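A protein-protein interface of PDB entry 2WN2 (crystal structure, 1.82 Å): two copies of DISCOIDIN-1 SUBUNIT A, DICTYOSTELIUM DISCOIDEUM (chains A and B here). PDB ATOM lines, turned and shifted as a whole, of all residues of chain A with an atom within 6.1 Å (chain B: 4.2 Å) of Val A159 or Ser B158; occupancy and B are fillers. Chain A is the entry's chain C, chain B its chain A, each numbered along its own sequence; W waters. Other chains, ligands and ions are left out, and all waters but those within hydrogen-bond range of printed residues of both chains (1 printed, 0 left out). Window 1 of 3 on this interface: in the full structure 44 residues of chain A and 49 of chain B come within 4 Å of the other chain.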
ATOM      1  N   SER A 157       2.798   9.224  22.829  1.00  0.00           N
ATOM      2  CA  SER A 157       4.047   9.574  22.190  1.00  0.00           C
ATOM      3  C   SER A 157       3.725  10.032  20.771  1.00  0.00           C
ATOM      4  O   SER A 157       3.015   9.323  20.048  1.00  0.00           O
ATOM      5  CB  SER A 157       4.974   8.360  22.089  1.00  0.00           C
ATOM      6  OG  SER A 157       6.251   8.755  21.555  1.00  0.00           O
ATOM      7  N   SER A 158       4.193  11.207  20.393  1.00  0.00           N
ATOM      8  CA  SER A 158       4.039  11.674  19.021  1.00  0.00           C
ATOM      9  C   SER A 158       5.394  11.884  18.327  1.00  0.00           C
ATOM     10  O   SER A 158       6.400  12.168  18.960  1.00  0.00           O
ATOM     11  CB  SER A 158       3.224  12.979  18.993  1.00  0.00           C
ATOM     12  OG  SER A 158       3.903  13.994  19.668  1.00  0.00           O
ATOM     13  N   VAL A 159       5.405  11.735  17.006  1.00  0.00           N
ATOM     14  CA  VAL A 159       6.551  12.118  16.206  1.00  0.00           C
ATOM     15  C   VAL A 159       6.056  13.057  15.118  1.00  0.00           C
ATOM     16  O   VAL A 159       5.060  12.779  14.453  1.00  0.00           O
ATOM     17  CB  VAL A 159       7.231  10.924  15.592  1.00  0.00           C
ATOM     18  CG1 VAL A 159       8.449  11.412  14.742  1.00  0.00           C
ATOM     19  CG2 VAL A 159       7.734   9.954  16.763  1.00  0.00           C
ATOM     20  N   THR A 160       6.721  14.177  14.977  1.00  0.00           N
ATOM     21  CA  THR A 160       6.292  15.227  14.034  1.00  0.00           C
ATOM     22  C   THR A 160       7.413  15.572  13.054  1.00  0.00           C
ATOM     23  O   THR A 160       8.630  15.650  13.437  1.00  0.00           O
ATOM     24  CB  THR A 160       5.923  16.494  14.833  1.00  0.00           C
ATOM     25  OG1 THR A 160       4.843  16.175  15.691  1.00  0.00           O
ATOM     26  CG2 THR A 160       5.568  17.696  13.915  1.00  0.00           C
ATOM     27  N   GLN A 161       7.033  15.786  11.795  1.00  0.00           N
ATOM     28  CA  GLN A 161       7.929  16.312  10.808  1.00  0.00           C
ATOM     29  C   GLN A 161       7.291  17.570  10.197  1.00  0.00           C
ATOM     30  O   GLN A 161       6.123  17.532   9.830  1.00  0.00           O
ATOM     31  CB  GLN A 161       8.197  15.295   9.703  1.00  0.00           C
ATOM     32  CG  GLN A 161       8.819  13.983  10.237  1.00  0.00           C
ATOM     33  CD  GLN A 161       9.234  13.072   9.132  1.00  0.00           C
ATOM     34  OE1 GLN A 161      10.120  13.409   8.347  1.00  0.00           O
ATOM     35  NE2 GLN A 161       8.615  11.904   9.070  1.00  0.00           N
ATOM     36  N   PHE A 191      11.798  11.183   6.751  1.00  0.00           N
ATOM     37  CA  PHE A 191      11.797   9.757   7.104  1.00  0.00           C
ATOM     38  C   PHE A 191      10.401   9.186   7.131  1.00  0.00           C
ATOM     39  O   PHE A 191       9.414   9.918   7.242  1.00  0.00           O
ATOM     40  CB  PHE A 191      12.526   9.509   8.410  1.00  0.00           C
ATOM     41  CG  PHE A 191      11.867  10.122   9.591  1.00  0.00           C
ATOM     42  CD1 PHE A 191      10.838   9.457  10.265  1.00  0.00           C
ATOM     43  CD2 PHE A 191      12.255  11.385  10.028  1.00  0.00           C
ATOM     44  CE1 PHE A 191      10.208  10.034  11.381  1.00  0.00           C
ATOM     45  CE2 PHE A 191      11.631  11.957  11.149  1.00  0.00           C
ATOM     46  CZ  PHE A 191      10.603  11.290  11.813  1.00  0.00           C
ATOM     47  N   PHE A 193       7.306   7.476   8.691  1.00  0.00           N
ATOM     48  CA  PHE A 193       6.668   7.336   9.997  1.00  0.00           C
ATOM     49  C   PHE A 193       6.360   5.862  10.302  1.00  0.00           C
ATOM     50  O   PHE A 193       6.031   5.076   9.390  1.00  0.00           O
ATOM     51  CB  PHE A 193       5.355   8.100  10.049  1.00  0.00           C
ATOM     52  CG  PHE A 193       5.486   9.608  10.091  1.00  0.00           C
ATOM     53  CD1 PHE A 193       5.793  10.242  11.276  1.00  0.00           C
ATOM     54  CD2 PHE A 193       5.177  10.387   8.962  1.00  0.00           C
ATOM     55  CE1 PHE A 193       5.854  11.644  11.352  1.00  0.00           C
ATOM     56  CE2 PHE A 193       5.206  11.799   9.024  1.00  0.00           C
ATOM     57  CZ  PHE A 193       5.530  12.428  10.232  1.00  0.00           C
ATOM     58  N   ALA A 250       3.231  17.202   9.857  1.00  0.00           N
ATOM     59  CA  ALA A 250       2.742  15.839   9.844  1.00  0.00           C
ATOM     60  C   ALA A 250       3.141  15.195  11.181  1.00  0.00           C
ATOM     61  O   ALA A 250       4.304  15.234  11.548  1.00  0.00           O
ATOM     62  CB  ALA A 250       3.352  15.037   8.634  1.00  0.00           C
ATOM     63  N   THR A 251       2.159  14.590  11.860  1.00  0.00           N
ATOM     64  CA  THR A 251       2.354  14.012  13.184  1.00  0.00           C
ATOM     65  C   THR A 251       1.749  12.638  13.227  1.00  0.00           C
ATOM     66  O   THR A 251       0.578  12.448  12.880  1.00  0.00           O
ATOM     67  CB  THR A 251       1.740  14.892  14.283  1.00  0.00           C
ATOM     68  OG1 THR A 251       2.367  16.199  14.238  1.00  0.00           O
ATOM     69  CG2 THR A 251       2.036  14.313  15.626  1.00  0.00           C
ATOM     70  N   ALA A 252       2.537  11.696  13.740  1.00  0.00           N
ATOM     71  CA  ALA A 252       2.074  10.307  13.911  1.00  0.00           C
ATOM     72  C   ALA A 252       2.060  10.018  15.415  1.00  0.00           C
ATOM     73  O   ALA A 252       2.929  10.535  16.157  1.00  0.00           O
ATOM     74  CB  ALA A 252       3.044   9.311  13.176  1.00  0.00           C
ATOM     75  N   LEU A 253       1.097   9.196  15.843  1.00  0.00           N
ATOM     76  CA  LEU A 253       0.933   8.855  17.254  1.00  0.00           C
ATOM     77  C   LEU A 253       1.264   7.401  17.575  1.00  0.00           C
ATOM     78  O   LEU A 253       1.030   6.488  16.773  1.00  0.00           O
ATOM     79  CB  LEU A 253      -0.504   9.140  17.730  1.00  0.00           C
ATOM     80  CG  LEU A 253      -1.101  10.539  17.606  1.00  0.00           C
ATOM     81  CD1 LEU A 253      -2.505  10.485  18.168  1.00  0.00           C
ATOM     82  CD2 LEU A 253      -0.291  11.597  18.331  1.00  0.00           C
ATOM     83  N   GLU A 254       1.813   7.211  18.771  1.00  0.00           N
ATOM     84  CA  GLU A 254       2.071   5.901  19.333  1.00  0.00           C
ATOM     85  C   GLU A 254       2.887   5.010  18.393  1.00  0.00           C
ATOM     86  O   GLU A 254       2.557   3.797  18.226  1.00  0.00           O
ATOM     87  CB  GLU A 254       0.765   5.274  19.762  1.00  0.00           C
ATOM     88  CG  GLU A 254       0.158   6.038  20.972  1.00  0.00           C
ATOM     89  CD  GLU A 254       0.888   5.745  22.272  1.00  0.00           C
ATOM     90  OE1 GLU A 254       0.544   4.719  22.903  1.00  0.00           O
ATOM     91  OE2 GLU A 254       1.774   6.536  22.659  1.00  0.00           O
ATOM     92  OXT GLU A 254       3.855   5.557  17.812  1.00  0.00           O
ATOM     93  N   GLN B 156      12.727   7.422  15.711  1.00  0.00           N
ATOM     94  CA  GLN B 156      13.084   8.820  15.552  1.00  0.00           C
ATOM     95  C   GLN B 156      12.372   9.600  16.626  1.00  0.00           C
ATOM     96  O   GLN B 156      11.247   9.262  17.007  1.00  0.00           O
ATOM     97  CB  GLN B 156      12.714   9.339  14.177  1.00  0.00           C
ATOM     98  CG  GLN B 156      13.588   8.768  13.081  1.00  0.00           C
ATOM     99  CD  GLN B 156      13.171   7.374  12.677  1.00  0.00           C
ATOM    100  OE1 GLN B 156      12.016   6.980  12.875  1.00  0.00           O
ATOM    101  NE2 GLN B 156      14.101   6.616  12.101  1.00  0.00           N
ATOM    102  N   SER B 157      13.049  10.610  17.143  1.00  0.00           N
ATOM    103  CA  SER B 157      12.480  11.436  18.188  1.00  0.00           C
ATOM    104  C   SER B 157      12.399  12.895  17.701  1.00  0.00           C
ATOM    105  O   SER B 157      13.408  13.450  17.253  1.00  0.00           O
ATOM    106  CB  SER B 157      13.408  11.415  19.392  1.00  0.00           C
ATOM    107  OG  SER B 157      12.783  12.086  20.484  1.00  0.00           O
ATOM    108  N   SER B 158      11.266  13.535  17.866  1.00  0.00           N
ATOM    109  CA  SER B 158      11.150  14.973  17.551  1.00  0.00           C
ATOM    110  C   SER B 158      10.774  15.757  18.789  1.00  0.00           C
ATOM    111  O   SER B 158      10.153  15.204  19.708  1.00  0.00           O
ATOM    112  CB  SER B 158      10.095  15.189  16.484  1.00  0.00           C
ATOM    113  OG  SER B 158       8.842  14.756  16.916  1.00  0.00           O
ATOM    114  N   VAL B 159      11.154  17.045  18.820  1.00  0.00           N
ATOM    115  CA  VAL B 159      10.690  17.980  19.837  1.00  0.00           C
ATOM    116  C   VAL B 159      10.094  19.167  19.054  1.00  0.00           C
ATOM    117  O   VAL B 159      10.703  19.633  18.071  1.00  0.00           O
ATOM    118  CB  VAL B 159      11.790  18.505  20.719  1.00  0.00           C
ATOM    119  CG1 VAL B 159      11.200  19.510  21.694  1.00  0.00           C
ATOM    120  CG2 VAL B 159      12.430  17.290  21.481  1.00  0.00           C
ATOM    121  N   THR B 251      10.059  22.289  14.680  1.00  0.00           N
ATOM    122  CA  THR B 251      10.316  20.903  15.091  1.00  0.00           C
ATOM    123  C   THR B 251      11.753  20.516  14.775  1.00  0.00           C
ATOM    124  O   THR B 251      12.222  20.739  13.658  1.00  0.00           O
ATOM    125  CB  THR B 251       9.397  19.905  14.403  1.00  0.00           C
ATOM    126  OG1 THR B 251       8.037  20.255  14.671  1.00  0.00           O
ATOM    127  CG2 THR B 251       9.647  18.465  14.953  1.00  0.00           C
ATOM    128  N   ALA B 252      12.457  19.995  15.802  1.00  0.00           N
ATOM    129  CA  ALA B 252      13.833  19.459  15.625  1.00  0.00           C
ATOM    130  C   ALA B 252      13.792  17.947  15.834  1.00  0.00           C
ATOM    131  O   ALA B 252      13.041  17.423  16.669  1.00  0.00           O
ATOM    132  CB  ALA B 252      14.829  20.076  16.647  1.00  0.00           C
ATOM    133  N   LEU B 253      14.659  17.267  15.096  1.00  0.00           N
ATOM    134  CA  LEU B 253      14.767  15.833  15.114  1.00  0.00           C
ATOM    135  C   LEU B 253      16.040  15.367  15.827  1.00  0.00           C
ATOM    136  O   LEU B 253      17.115  15.988  15.721  1.00  0.00           O
ATOM    137  CB  LEU B 253      14.816  15.323  13.689  1.00  0.00           C
ATOM    138  CG  LEU B 253      13.508  15.485  12.932  1.00  0.00           C
ATOM    139  CD1 LEU B 253      13.735  15.004  11.515  1.00  0.00           C
ATOM    140  CD2 LEU B 253      12.407  14.707  13.619  1.00  0.00           C
HETATM  141  O   HOH W   1       8.988  12.321  19.519  1.00  0.00           O
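OG of Ser B158 is in hydrogen-bond range of N of Thr A160.
The backbone carbonyl oxygen (O) of Val A159 sits at hydrogen-bond distance from the backbone NH (N) of Ala A252, 2.8 Å away.
The side-chain hydroxyl (OG1) of Thr A251 lies within hydrogen-bond range of the side-chain hydroxyl (OG1) of Thr A160.
NE2 of Gln A161 is in hydrogen-bond range of O of Phe A191, 2.8 Å away.
Gln B156 touches Val A159 (O to CG2, 3.6 Å).
CA of Val A159 touches OG of Ser B158, at 3.6 Å.
CG2 of Thr B251 touches O of Thr A160, 3.4 Å away.
Leu B253 touches Thr A160.
CZ of Phe A191 touches CB of Gln B156, at 3.7 Å.
Phe A191 touches Leu B253 (CE2 to CD1, 3.7 Å).
Ser A157 touches none of the printed residues of chain B.
Of the printed residues of chain B, Thr A160 touches Ser B158, Thr B251 and Leu B253.
Of the printed residues of chain B, Phe A191 touches Gln B156 and Leu B253.
Of the printed residues of chain A, Gln B156 touches Val A159 (3.6 Å) and Phe A191 (3.7 Å).
Ser B158 touches just these residues of chain A: Val A159 and Thr A160.
The nearest printed residue of chain B that does not touch Phe A191 is Ser B157 (5.9 Å).
Hydrophobic or aromatic side chains of chain A within 4 Å of the printed part of chain B: Val A159 and Phe A191.
Hydrophobic or aromatic side chains of chain B that line the printed part of chain A: Leu B253.
Along chain B the printed residues that touch a printed residue of chain A span positions 156 to 253.
Among the printed residues, 7 pairs touch across the chains.
Among the printed residues, no Asp or Glu carboxylate lies within 4 Å of a Lys or Arg side-chain nitrogen of the other chain.
Val A159 touches Ser B158, but with the chains exchanged Ser A158 does not touch Val B159 (6.8 Å).
Positions printed for both chains: 157, 158, 159, 251, 252 and 253.
Of the 7 pairs that touch across the chains among the printed residues, none has its exchanged pair printed and touching as well.
Water W1 bridges O of Ser A158 (2.7 Å) and N of Ser B158 (3.1 Å).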
